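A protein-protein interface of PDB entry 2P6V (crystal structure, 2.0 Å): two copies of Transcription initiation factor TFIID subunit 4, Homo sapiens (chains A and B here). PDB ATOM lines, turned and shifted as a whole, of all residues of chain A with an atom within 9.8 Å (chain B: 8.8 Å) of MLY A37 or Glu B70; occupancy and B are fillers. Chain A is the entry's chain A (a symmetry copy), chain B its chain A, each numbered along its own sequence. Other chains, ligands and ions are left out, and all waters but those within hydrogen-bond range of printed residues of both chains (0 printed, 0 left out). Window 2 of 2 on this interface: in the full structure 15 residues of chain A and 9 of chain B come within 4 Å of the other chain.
Of the printed residues of chain B, MLY A37 touches Arg B69 (3.5 Å) and Glu B70 (3.8 Å).
Of chain A, only MLY A37 comes within 4 Å of Glu B70.
No residue of chain B comes within 4 Å of Gly A36.
No residue of chain A comes within 4 Å of Asn B45.
No residue of chain A comes within 4 Å of Leu B71.
Of the printed residues of chain A, Asn B72 touches Gln A38.
Of the printed residues of chain A, Arg B69 touches MLY A31 (3.0 Å), Leu A32 (3.2 Å), Ser A35 (3.6 Å) and MLY A37 (3.5 Å).
Of the printed residues of chain B, Gln A38 touches Asn B72 (3.3 Å).
Of the printed residues of chain A, Ser B73 touches Leu A32.
Of the printed residues of chain B, MLY A31 touches Arg B69.
The nearest printed residue of chain B that does not touch MLY A37 is Thr B42 (5.4 Å).
The nearest residue of chain A that does not touch Glu B70 is Leu A32 (6.6 Å).
Positions printed for both chains: 33, 38, 39, 40, 41, 42 and 43.
MLY A31 touches Arg B69 (CB to NH2, 3.0 Å).
Leu A32 touches Arg B69 (CD2 to CG, 3.2 Å).
Leu A32 touches Ser B73 (CD1 to O, 3.5 Å).
Ser A35 touches Arg B69.
MLY A37 touches Glu B70 (CH1 to O, 3.8 Å).
Hydrophobic or aromatic side chains of chain A within 4 Å of the printed part of chain B: Leu A32.
Among the printed residues, 7 pairs touch across the chains.
Among the printed residues, no Asp or Glu carboxylate lies within 4 Å of a Lys or Arg side-chain nitrogen of the other chain.
The backbone carbonyl oxygen (O) of Arg B69 lies close to NZ of MLY A37 (3.5 Å).
OD1 of Asn B72 sits at hydrogen-bond distance from NE2 of Gln A38 (3.3 Å).
OG1 of Thr B42 sits close to OE2 of Glu B70.
The side-chain carboxylate (OE2) of Glu B70 is in hydrogen-bond range of the side-chain amide nitrogen (ND2) of Asn B45 (3.0 Å).
The backbone NH (N) of Ser B73 sits at hydrogen-bond distance from the backbone carbonyl oxygen (O) of Tyr B68 (2.8 Å).
The side-chain hydroxyl of Ser A35 is in hydrogen-bond range of the backbone carbonyl oxygen of Leu A32, at 3.0 Å.
The side-chain hydroxyl (OG) of Ser A35 sits close to N of MLY A37, at 3.3 Å.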
ATOM      1  N   ILE A  30       4.649  -3.315 -21.271  1.00  0.00           N
ATOM      2  CA  ILE A  30       3.446  -3.061 -20.466  1.00  0.00           C
ATOM      3  C   ILE A  30       2.175  -3.479 -21.204  1.00  0.00           C
ATOM      4  O   ILE A  30       1.279  -4.102 -20.612  1.00  0.00           O
ATOM      5  CB  ILE A  30       3.290  -1.558 -20.123  1.00  0.00           C
ATOM      6  CG1 ILE A  30       4.419  -1.091 -19.198  1.00  0.00           C
ATOM      7  CG2 ILE A  30       1.929  -1.264 -19.487  1.00  0.00           C
ATOM      8  CD1 ILE A  30       4.614  -1.892 -18.005  1.00  0.00           C
ATOM      9  N   MLY A  31       2.053  -3.104 -22.477  1.00  0.00           N
ATOM     10  CA  MLY A  31       0.905  -3.502 -23.295  1.00  0.00           C
ATOM     11  CB  MLY A  31       0.965  -2.981 -24.738  1.00  0.00           C
ATOM     12  CG  MLY A  31       0.982  -1.458 -24.858  1.00  0.00           C
ATOM     13  CD  MLY A  31       1.056  -1.012 -26.316  1.00  0.00           C
ATOM     14  CE  MLY A  31       2.059   0.103 -26.634  1.00  0.00           C
ATOM     15  NZ  MLY A  31       2.801  -0.269 -27.863  1.00  0.00           N
ATOM     16  CH1 MLY A  31       1.970  -0.079 -29.073  1.00  0.00           C
ATOM     17  CH2 MLY A  31       4.051   0.508 -27.963  1.00  0.00           C
ATOM     18  C   MLY A  31       0.737  -4.994 -23.374  1.00  0.00           C
ATOM     19  O   MLY A  31      -0.365  -5.524 -23.227  1.00  0.00           O
ATOM     20  N   LEU A  32       1.834  -5.698 -23.620  1.00  0.00           N
ATOM     21  CA  LEU A  32       1.805  -7.164 -23.662  1.00  0.00           C
ATOM     22  C   LEU A  32       1.362  -7.699 -22.313  1.00  0.00           C
ATOM     23  O   LEU A  32       0.509  -8.560 -22.254  1.00  0.00           O
ATOM     24  CB  LEU A  32       3.177  -7.771 -23.987  1.00  0.00           C
ATOM     25  CG  LEU A  32       3.635  -7.412 -25.415  1.00  0.00           C
ATOM     26  CD1 LEU A  32       5.055  -7.806 -25.703  1.00  0.00           C
ATOM     27  CD2 LEU A  32       2.718  -8.089 -26.424  1.00  0.00           C
ATOM     28  N   ALA A  33       1.968  -7.199 -21.243  1.00  0.00           N
ATOM     29  CA  ALA A  33       1.720  -7.736 -19.905  1.00  0.00           C
ATOM     30  C   ALA A  33       0.312  -7.510 -19.390  1.00  0.00           C
ATOM     31  O   ALA A  33      -0.206  -8.306 -18.616  1.00  0.00           O
ATOM     32  CB  ALA A  33       2.760  -7.221 -18.924  1.00  0.00           C
ATOM     33  N   SER A  34      -0.272  -6.417 -19.855  1.00  0.00           N
ATOM     34  CA  SER A  34      -1.602  -5.946 -19.538  1.00  0.00           C
ATOM     35  C   SER A  34      -2.652  -6.445 -20.524  1.00  0.00           C
ATOM     36  O   SER A  34      -3.801  -6.025 -20.436  1.00  0.00           O
ATOM     37  CB  SER A  34      -1.590  -4.400 -19.519  1.00  0.00           C
ATOM     38  OG  SER A  34      -0.687  -3.944 -18.509  1.00  0.00           O
ATOM     39  N   SER A  35      -2.321  -7.328 -21.461  1.00  0.00           N
ATOM     40  CA  SER A  35      -3.330  -7.662 -22.470  1.00  0.00           C
ATOM     41  C   SER A  35      -4.413  -8.628 -21.973  1.00  0.00           C
ATOM     42  O   SER A  35      -5.425  -8.834 -22.649  1.00  0.00           O
ATOM     43  CB  SER A  35      -2.702  -8.299 -23.704  1.00  0.00           C
ATOM     44  OG  SER A  35      -2.124  -9.533 -23.333  1.00  0.00           O
ATOM     45  N   GLY A  36      -4.234  -9.269 -20.825  1.00  0.00           N
ATOM     46  CA  GLY A  36      -5.244 -10.269 -20.456  1.00  0.00           C
ATOM     47  C   GLY A  36      -5.127 -11.606 -21.181  1.00  0.00           C
ATOM     48  O   GLY A  36      -5.970 -12.476 -21.025  1.00  0.00           O
ATOM     49  N   MLY A  37      -4.097 -11.802 -21.993  1.00  0.00           N
ATOM     50  CA  MLY A  37      -3.730 -13.149 -22.402  1.00  0.00           C
ATOM     51  CB  MLY A  37      -3.083 -13.216 -23.785  1.00  0.00           C
ATOM     52  CG  MLY A  37      -4.000 -12.974 -24.986  1.00  0.00           C
ATOM     53  CD  MLY A  37      -3.252 -13.219 -26.303  1.00  0.00           C
ATOM     54  CE  MLY A  37      -3.266 -14.673 -26.797  1.00  0.00           C
ATOM     55  NZ  MLY A  37      -2.515 -14.859 -28.062  1.00  0.00           N
ATOM     56  CH1 MLY A  37      -1.891 -16.196 -28.114  1.00  0.00           C
ATOM     57  CH2 MLY A  37      -3.395 -14.664 -29.230  1.00  0.00           C
ATOM     58  C   MLY A  37      -2.710 -13.595 -21.387  1.00  0.00           C
ATOM     59  O   MLY A  37      -2.234 -14.724 -21.448  1.00  0.00           O
ATOM     60  N   GLN A  38      -2.353 -12.719 -20.442  1.00  0.00           N
ATOM     61  CA  GLN A  38      -1.298 -13.005 -19.465  1.00  0.00           C
ATOM     62  C   GLN A  38      -1.764 -13.146 -18.014  1.00  0.00           C
ATOM     63  O   GLN A  38      -2.822 -12.621 -17.659  1.00  0.00           O
ATOM     64  CB  GLN A  38      -0.275 -11.850 -19.496  1.00  0.00           C
ATOM     65  CG  GLN A  38       0.788 -11.963 -20.554  1.00  0.00           C
ATOM     66  CD  GLN A  38       1.583 -13.217 -20.305  1.00  0.00           C
ATOM     67  OE1 GLN A  38       2.492 -13.251 -19.468  1.00  0.00           O
ATOM     68  NE2 GLN A  38       1.221 -14.280 -21.014  1.00  0.00           N
ATOM     69  N   SER A  39      -0.964 -13.784 -17.161  1.00  0.00           N
ATOM     70  CA  SER A  39      -1.413 -13.978 -15.767  1.00  0.00           C
ATOM     71  C   SER A  39      -1.426 -12.673 -14.997  1.00  0.00           C
ATOM     72  O   SER A  39      -0.580 -11.824 -15.198  1.00  0.00           O
ATOM     73  CB  SER A  39      -0.601 -15.074 -15.062  1.00  0.00           C
ATOM     74  OG  SER A  39       0.442 -14.610 -14.233  1.00  0.00           O
ATOM     75  N   THR A  40      -2.398 -12.476 -14.124  1.00  0.00           N
ATOM     76  CA  THR A  40      -2.546 -11.185 -13.437  1.00  0.00           C
ATOM     77  C   THR A  40      -1.284 -10.808 -12.613  1.00  0.00           C
ATOM     78  O   THR A  40      -0.916  -9.643 -12.460  1.00  0.00           O
ATOM     79  CB  THR A  40      -3.859 -11.186 -12.574  1.00  0.00           C
ATOM     80  OG1 THR A  40      -4.644 -10.017 -12.835  1.00  0.00           O
ATOM     81  CG2 THR A  40      -3.598 -11.235 -11.074  1.00  0.00           C
ATOM     82  N   GLU A  41      -0.635 -11.828 -12.078  1.00  0.00           N
ATOM     83  CA  GLU A  41       0.597 -11.742 -11.311  1.00  0.00           C
ATOM     84  C   GLU A  41       1.792 -11.332 -12.182  1.00  0.00           C
ATOM     85  O   GLU A  41       2.626 -10.522 -11.812  1.00  0.00           O
ATOM     86  CB  GLU A  41       0.795 -13.149 -10.778  1.00  0.00           C
ATOM     87  CG  GLU A  41       1.899 -13.506  -9.819  1.00  0.00           C
ATOM     88  CD  GLU A  41       1.511 -14.825  -9.159  1.00  0.00           C
ATOM     89  OE1 GLU A  41       0.665 -14.785  -8.224  1.00  0.00           O
ATOM     90  OE2 GLU A  41       2.015 -15.887  -9.604  1.00  0.00           O
ATOM     91  N   THR A  42       1.911 -11.931 -13.352  1.00  0.00           N
ATOM     92  CA  THR A  42       2.901 -11.496 -14.341  1.00  0.00           C
ATOM     93  C   THR A  42       2.759 -10.018 -14.703  1.00  0.00           C
ATOM     94  O   THR A  42       3.724  -9.251 -14.694  1.00  0.00           O
ATOM     95  CB  THR A  42       2.773 -12.334 -15.614  1.00  0.00           C
ATOM     96  OG1 THR A  42       3.289 -13.642 -15.334  1.00  0.00           O
ATOM     97  CG2 THR A  42       3.555 -11.687 -16.765  1.00  0.00           C
ATOM     98  N   ALA A  43       1.544  -9.607 -15.026  1.00  0.00           N
ATOM     99  CA  ALA A  43       1.316  -8.234 -15.330  1.00  0.00           C
ATOM    100  C   ALA A  43       1.716  -7.280 -14.235  1.00  0.00           C
ATOM    101  O   ALA A  43       2.253  -6.211 -14.502  1.00  0.00           O
ATOM    102  CB  ALA A  43      -0.141  -7.992 -15.664  1.00  0.00           C
ATOM    103  N   ALA B  33       6.722 -22.045 -36.532  1.00  0.00           N
ATOM    104  CA  ALA B  33       5.264 -22.000 -36.429  1.00  0.00           C
ATOM    105  C   ALA B  33       4.558 -23.223 -36.980  1.00  0.00           C
ATOM    106  O   ALA B  33       3.490 -23.595 -36.510  1.00  0.00           O
ATOM    107  CB  ALA B  33       4.726 -20.722 -37.049  1.00  0.00           C
ATOM    108  N   GLN B  38       3.402 -26.417 -32.101  1.00  0.00           N
ATOM    109  CA  GLN B  38       2.629 -25.181 -31.956  1.00  0.00           C
ATOM    110  C   GLN B  38       1.138 -25.292 -32.290  1.00  0.00           C
ATOM    111  O   GLN B  38       0.746 -26.195 -33.034  1.00  0.00           O
ATOM    112  CB  GLN B  38       3.221 -24.118 -32.906  1.00  0.00           C
ATOM    113  CG  GLN B  38       4.393 -23.351 -32.358  1.00  0.00           C
ATOM    114  CD  GLN B  38       3.949 -22.608 -31.126  1.00  0.00           C
ATOM    115  OE1 GLN B  38       3.350 -21.529 -31.202  1.00  0.00           O
ATOM    116  NE2 GLN B  38       4.210 -23.203 -29.968  1.00  0.00           N
ATOM    117  N   SER B  39       0.321 -24.356 -31.811  1.00  0.00           N
ATOM    118  CA  SER B  39      -1.129 -24.469 -32.077  1.00  0.00           C
ATOM    119  C   SER B  39      -1.452 -24.206 -33.535  1.00  0.00           C
ATOM    120  O   SER B  39      -0.831 -23.377 -34.169  1.00  0.00           O
ATOM    121  CB  SER B  39      -1.946 -23.589 -31.121  1.00  0.00           C
ATOM    122  OG  SER B  39      -2.358 -22.348 -31.651  1.00  0.00           O
ATOM    123  N   THR B  40      -2.409 -24.923 -34.098  1.00  0.00           N
ATOM    124  CA  THR B  40      -2.687 -24.812 -35.537  1.00  0.00           C
ATOM    125  C   THR B  40      -3.075 -23.366 -35.952  1.00  0.00           C
ATOM    126  O   THR B  40      -2.787 -22.893 -37.052  1.00  0.00           O
ATOM    127  CB  THR B  40      -3.765 -25.875 -35.956  1.00  0.00           C
ATOM    128  OG1 THR B  40      -3.333 -26.618 -37.103  1.00  0.00           O
ATOM    129  CG2 THR B  40      -5.119 -25.265 -36.292  1.00  0.00           C
ATOM    130  N   GLU B  41      -3.745 -22.679 -35.043  1.00  0.00           N
ATOM    131  CA  GLU B  41      -4.174 -21.297 -35.169  1.00  0.00           C
ATOM    132  C   GLU B  41      -2.989 -20.320 -35.152  1.00  0.00           C
ATOM    133  O   GLU B  41      -2.914 -19.368 -35.912  1.00  0.00           O
ATOM    134  CB  GLU B  41      -5.054 -21.073 -33.953  1.00  0.00           C
ATOM    135  CG  GLU B  41      -5.822 -19.799 -33.730  1.00  0.00           C
ATOM    136  CD  GLU B  41      -6.916 -20.107 -32.712  1.00  0.00           C
ATOM    137  OE1 GLU B  41      -7.951 -20.698 -33.128  1.00  0.00           O
ATOM    138  OE2 GLU B  41      -6.719 -19.799 -31.511  1.00  0.00           O
ATOM    139  N   THR B  42      -2.058 -20.529 -34.240  1.00  0.00           N
ATOM    140  CA  THR B  42      -0.799 -19.778 -34.243  1.00  0.00           C
ATOM    141  C   THR B  42      -0.045 -19.900 -35.567  1.00  0.00           C
ATOM    142  O   THR B  42       0.380 -18.911 -36.166  1.00  0.00           O
ATOM    143  CB  THR B  42       0.104 -20.267 -33.109  1.00  0.00           C
ATOM    144  OG1 THR B  42      -0.445 -19.789 -31.873  1.00  0.00           O
ATOM    145  CG2 THR B  42       1.533 -19.741 -33.296  1.00  0.00           C
ATOM    146  N   ALA B  43       0.124 -21.126 -36.035  1.00  0.00           N
ATOM    147  CA  ALA B  43       0.775 -21.325 -37.285  1.00  0.00           C
ATOM    148  C   ALA B  43       0.130 -20.608 -38.442  1.00  0.00           C
ATOM    149  O   ALA B  43       0.814 -20.079 -39.310  1.00  0.00           O
ATOM    150  CB  ALA B  43       0.854 -22.800 -37.622  1.00  0.00           C
ATOM    151  N   ALA B  44      -1.192 -20.603 -38.484  1.00  0.00           N
ATOM    152  CA  ALA B  44      -1.855 -19.951 -39.598  1.00  0.00           C
ATOM    153  C   ALA B  44      -1.661 -18.462 -39.432  1.00  0.00           C
ATOM    154  O   ALA B  44      -1.613 -17.712 -40.411  1.00  0.00           O
ATOM    155  CB  ALA B  44      -3.346 -20.271 -39.591  1.00  0.00           C
ATOM    156  N   ASN B  45      -1.569 -18.016 -38.182  1.00  0.00           N
ATOM    157  CA  ASN B  45      -1.529 -16.584 -37.952  1.00  0.00           C
ATOM    158  C   ASN B  45      -0.140 -16.003 -38.284  1.00  0.00           C
ATOM    159  O   ASN B  45      -0.040 -14.884 -38.792  1.00  0.00           O
ATOM    160  CB  ASN B  45      -1.913 -16.281 -36.499  1.00  0.00           C
ATOM    161  CG  ASN B  45      -3.407 -16.498 -36.219  1.00  0.00           C
ATOM    162  OD1 ASN B  45      -4.229 -16.434 -37.107  1.00  0.00           O
ATOM    163  ND2 ASN B  45      -3.752 -16.741 -34.977  1.00  0.00           N
ATOM    164  N   VAL B  46       0.896 -16.758 -37.920  1.00  0.00           N
ATOM    165  CA  VAL B  46       2.263 -16.375 -38.196  1.00  0.00           C
ATOM    166  C   VAL B  46       2.448 -16.427 -39.705  1.00  0.00           C
ATOM    167  O   VAL B  46       2.979 -15.492 -40.245  1.00  0.00           O
ATOM    168  CB  VAL B  46       3.282 -17.216 -37.409  1.00  0.00           C
ATOM    169  CG1 VAL B  46       4.742 -16.898 -37.837  1.00  0.00           C
ATOM    170  CG2 VAL B  46       3.111 -16.937 -35.942  1.00  0.00           C
ATOM    171  N   MLY B  47       2.001 -17.475 -40.398  1.00  0.00           N
ATOM    172  CA  MLY B  47       2.059 -17.508 -41.846  1.00  0.00           C
ATOM    173  CB  MLY B  47       1.354 -18.738 -42.426  1.00  0.00           C
ATOM    174  CG  MLY B  47       2.282 -19.945 -42.405  1.00  0.00           C
ATOM    175  CD  MLY B  47       1.596 -21.209 -42.928  1.00  0.00           C
ATOM    176  CE  MLY B  47       1.916 -22.489 -42.160  1.00  0.00           C
ATOM    177  NZ  MLY B  47       1.560 -23.665 -42.988  1.00  0.00           N
ATOM    178  CH1 MLY B  47       1.891 -24.905 -42.256  1.00  0.00           C
ATOM    179  CH2 MLY B  47       0.125 -23.632 -43.348  1.00  0.00           C
ATOM    180  C   MLY B  47       1.423 -16.303 -42.425  1.00  0.00           C
ATOM    181  O   MLY B  47       1.989 -15.690 -43.328  1.00  0.00           O
ATOM    182  N   GLU B  48       0.267 -15.895 -41.912  1.00  0.00           N
ATOM    183  CA  GLU B  48      -0.412 -14.724 -42.485  1.00  0.00           C
ATOM    184  C   GLU B  48       0.309 -13.424 -42.202  1.00  0.00           C
ATOM    185  O   GLU B  48       0.357 -12.561 -43.063  1.00  0.00           O
ATOM    186  CB  GLU B  48      -1.901 -14.571 -42.067  1.00  0.00           C
ATOM    187  CG  GLU B  48      -2.748 -14.198 -43.310  1.00  0.00           C
ATOM    188  CD  GLU B  48      -2.493 -15.168 -44.510  1.00  0.00           C
ATOM    189  OE1 GLU B  48      -2.151 -14.757 -45.653  1.00  0.00           O
ATOM    190  OE2 GLU B  48      -2.611 -16.396 -44.302  1.00  0.00           O
ATOM    191  N   LEU B  49       0.832 -13.247 -40.993  1.00  0.00           N
ATOM    192  CA  LEU B  49       1.707 -12.080 -40.744  1.00  0.00           C
ATOM    193  C   LEU B  49       2.916 -11.955 -41.701  1.00  0.00           C
ATOM    194  O   LEU B  49       3.198 -10.895 -42.250  1.00  0.00           O
ATOM    195  CB  LEU B  49       2.256 -12.176 -39.308  1.00  0.00           C
ATOM    196  CG  LEU B  49       1.238 -11.835 -38.209  1.00  0.00           C
ATOM    197  CD1 LEU B  49       1.803 -12.069 -36.819  1.00  0.00           C
ATOM    198  CD2 LEU B  49       0.838 -10.407 -38.353  1.00  0.00           C
ATOM    199  N   PHE B  63       3.788  -5.412 -37.830  1.00  0.00           N
ATOM    200  CA  PHE B  63       4.058  -6.820 -37.882  1.00  0.00           C
ATOM    201  C   PHE B  63       4.677  -7.268 -36.538  1.00  0.00           C
ATOM    202  O   PHE B  63       4.235  -8.303 -35.969  1.00  0.00           O
ATOM    203  CB  PHE B  63       4.963  -7.093 -39.086  1.00  0.00           C
ATOM    204  CG  PHE B  63       5.675  -8.403 -39.042  1.00  0.00           C
ATOM    205  CD1 PHE B  63       5.138  -9.525 -39.626  1.00  0.00           C
ATOM    206  CD2 PHE B  63       6.908  -8.498 -38.438  1.00  0.00           C
ATOM    207  CE1 PHE B  63       5.749 -10.708 -39.589  1.00  0.00           C
ATOM    208  CE2 PHE B  63       7.553  -9.711 -38.449  1.00  0.00           C
ATOM    209  CZ  PHE B  63       6.980 -10.792 -38.980  1.00  0.00           C
ATOM    210  N   THR B  64       5.664  -6.514 -36.043  1.00  0.00           N
ATOM    211  CA  THR B  64       6.357  -7.002 -34.815  1.00  0.00           C
ATOM    212  C   THR B  64       5.424  -6.980 -33.601  1.00  0.00           C
ATOM    213  O   THR B  64       5.397  -7.926 -32.809  1.00  0.00           O
ATOM    214  CB  THR B  64       7.634  -6.218 -34.478  1.00  0.00           C
ATOM    215  OG1 THR B  64       7.317  -4.841 -34.354  1.00  0.00           O
ATOM    216  CG2 THR B  64       8.618  -6.305 -35.605  1.00  0.00           C
ATOM    217  N   SER B  65       4.611  -5.929 -33.501  1.00  0.00           N
ATOM    218  CA  SER B  65       3.604  -5.858 -32.407  1.00  0.00           C
ATOM    219  C   SER B  65       2.679  -7.030 -32.393  1.00  0.00           C
ATOM    220  O   SER B  65       2.350  -7.608 -31.354  1.00  0.00           O
ATOM    221  CB  SER B  65       2.665  -4.663 -32.559  1.00  0.00           C
ATOM    222  OG  SER B  65       3.421  -3.480 -32.440  1.00  0.00           O
ATOM    223  N   ARG B  66       2.206  -7.400 -33.580  1.00  0.00           N
ATOM    224  CA  ARG B  66       1.301  -8.528 -33.673  1.00  0.00           C
ATOM    225  C   ARG B  66       1.940  -9.848 -33.490  1.00  0.00           C
ATOM    226  O   ARG B  66       1.313 -10.786 -33.035  1.00  0.00           O
ATOM    227  CB  ARG B  66       0.617  -8.583 -35.040  1.00  0.00           C
ATOM    228  CG  ARG B  66      -0.324  -7.414 -35.268  1.00  0.00           C
ATOM    229  CD  ARG B  66      -1.062  -7.636 -36.572  1.00  0.00           C
ATOM    230  NE  ARG B  66      -1.499  -6.388 -37.185  1.00  0.00           N
ATOM    231  CZ  ARG B  66      -2.727  -5.894 -37.071  1.00  0.00           C
ATOM    232  NH1 ARG B  66      -3.656  -6.530 -36.365  1.00  0.00           N
ATOM    233  NH2 ARG B  66      -3.024  -4.753 -37.673  1.00  0.00           N
ATOM    234  N   LEU B  67       3.203  -9.910 -33.877  1.00  0.00           N
ATOM    235  CA  LEU B  67       3.942 -11.138 -33.711  1.00  0.00           C
ATOM    236  C   LEU B  67       4.195 -11.426 -32.235  1.00  0.00           C
ATOM    237  O   LEU B  67       4.092 -12.549 -31.782  1.00  0.00           O
ATOM    238  CB  LEU B  67       5.299 -10.963 -34.437  1.00  0.00           C
ATOM    239  CG  LEU B  67       6.229 -12.174 -34.381  1.00  0.00           C
ATOM    240  CD1 LEU B  67       5.644 -13.275 -35.260  1.00  0.00           C
ATOM    241  CD2 LEU B  67       7.678 -11.873 -34.799  1.00  0.00           C
ATOM    242  N   TYR B  68       4.629 -10.413 -31.504  1.00  0.00           N
ATOM    243  CA  TYR B  68       4.922 -10.586 -30.062  1.00  0.00           C
ATOM    244  C   TYR B  68       3.676 -11.093 -29.314  1.00  0.00           C
ATOM    245  O   TYR B  68       3.711 -11.962 -28.451  1.00  0.00           O
ATOM    246  CB  TYR B  68       5.353  -9.278 -29.418  1.00  0.00           C
ATOM    247  CG  TYR B  68       6.580  -8.584 -29.945  1.00  0.00           C
ATOM    248  CD1 TYR B  68       7.679  -9.296 -30.373  1.00  0.00           C
ATOM    249  CD2 TYR B  68       6.680  -7.205 -29.904  1.00  0.00           C
ATOM    250  CE1 TYR B  68       8.800  -8.666 -30.837  1.00  0.00           C
ATOM    251  CE2 TYR B  68       7.815  -6.543 -30.360  1.00  0.00           C
ATOM    252  CZ  TYR B  68       8.856  -7.321 -30.863  1.00  0.00           C
ATOM    253  OH  TYR B  68      10.006  -6.699 -31.252  1.00  0.00           O
ATOM    254  N   ARG B  69       2.532 -10.557 -29.690  1.00  0.00           N
ATOM    255  CA  ARG B  69       1.225 -10.988 -29.157  1.00  0.00           C
ATOM    256  C   ARG B  69       0.925 -12.429 -29.553  1.00  0.00           C
ATOM    257  O   ARG B  69       0.494 -13.214 -28.722  1.00  0.00           O
ATOM    258  CB  ARG B  69       0.205  -9.869 -29.389  1.00  0.00           C
ATOM    259  CG  ARG B  69       0.651  -8.463 -28.815  1.00  0.00           C
ATOM    260  CD  ARG B  69      -0.189  -7.283 -29.329  1.00  0.00           C
ATOM    261  NE  ARG B  69      -0.092  -6.066 -28.542  1.00  0.00           N
ATOM    262  CZ  ARG B  69      -0.616  -5.949 -27.329  1.00  0.00           C
ATOM    263  NH1 ARG B  69      -1.251  -6.973 -26.740  1.00  0.00           N
ATOM    264  NH2 ARG B  69      -0.478  -4.789 -26.708  1.00  0.00           N
ATOM    265  N   GLU B  70       1.192 -12.801 -30.805  1.00  0.00           N
ATOM    266  CA  GLU B  70       0.809 -14.110 -31.312  1.00  0.00           C
ATOM    267  C   GLU B  70       1.623 -15.225 -30.690  1.00  0.00           C
ATOM    268  O   GLU B  70       1.116 -16.331 -30.450  1.00  0.00           O
ATOM    269  CB  GLU B  70       0.875 -14.139 -32.851  1.00  0.00           C
ATOM    270  CG  GLU B  70       0.263 -15.364 -33.496  1.00  0.00           C
ATOM    271  CD  GLU B  70      -1.211 -15.582 -33.122  1.00  0.00           C
ATOM    272  OE1 GLU B  70      -1.945 -14.570 -33.010  1.00  0.00           O
ATOM    273  OE2 GLU B  70      -1.592 -16.766 -32.958  1.00  0.00           O
ATOM    274  N   LEU B  71       2.880 -14.919 -30.427  1.00  0.00           N
ATOM    275  CA  LEU B  71       3.799 -15.921 -29.920  1.00  0.00           C
ATOM    276  C   LEU B  71       4.022 -15.708 -28.469  1.00  0.00           C
ATOM    277  O   LEU B  71       4.874 -16.391 -27.861  1.00  0.00           O
ATOM    278  CB  LEU B  71       5.183 -15.783 -30.565  1.00  0.00           C
ATOM    279  CG  LEU B  71       5.331 -15.871 -32.094  1.00  0.00           C
ATOM    280  CD1 LEU B  71       6.768 -15.556 -32.488  1.00  0.00           C
ATOM    281  CD2 LEU B  71       4.885 -17.220 -32.651  1.00  0.00           C
ATOM    282  N   ASN B  72       3.331 -14.714 -27.942  1.00  0.00           N
ATOM    283  CA  ASN B  72       3.579 -14.322 -26.573  1.00  0.00           C
ATOM    284  C   ASN B  72       5.071 -14.254 -26.383  1.00  0.00           C
ATOM    285  O   ASN B  72       5.654 -14.922 -25.532  1.00  0.00           O
ATOM    286  CB  ASN B  72       2.972 -15.316 -25.581  1.00  0.00           C
ATOM    287  CG  ASN B  72       3.133 -14.838 -24.163  1.00  0.00           C
ATOM    288  OD1 ASN B  72       2.803 -13.688 -23.868  1.00  0.00           O
ATOM    289  ND2 ASN B  72       3.656 -15.697 -23.286  1.00  0.00           N
ATOM    290  N   SER B  73       5.710 -13.445 -27.209  1.00  0.00           N
ATOM    291  CA  SER B  73       7.123 -13.213 -26.997  1.00  0.00           C
ATOM    292  C   SER B  73       7.387 -11.795 -26.523  1.00  0.00           C
ATOM    293  O   SER B  73       6.519 -10.925 -26.547  1.00  0.00           O
ATOM    294  CB  SER B  73       7.947 -13.506 -28.282  1.00  0.00           C
ATOM    295  OG  SER B  73       7.450 -12.842 -29.423  1.00  0.00           O
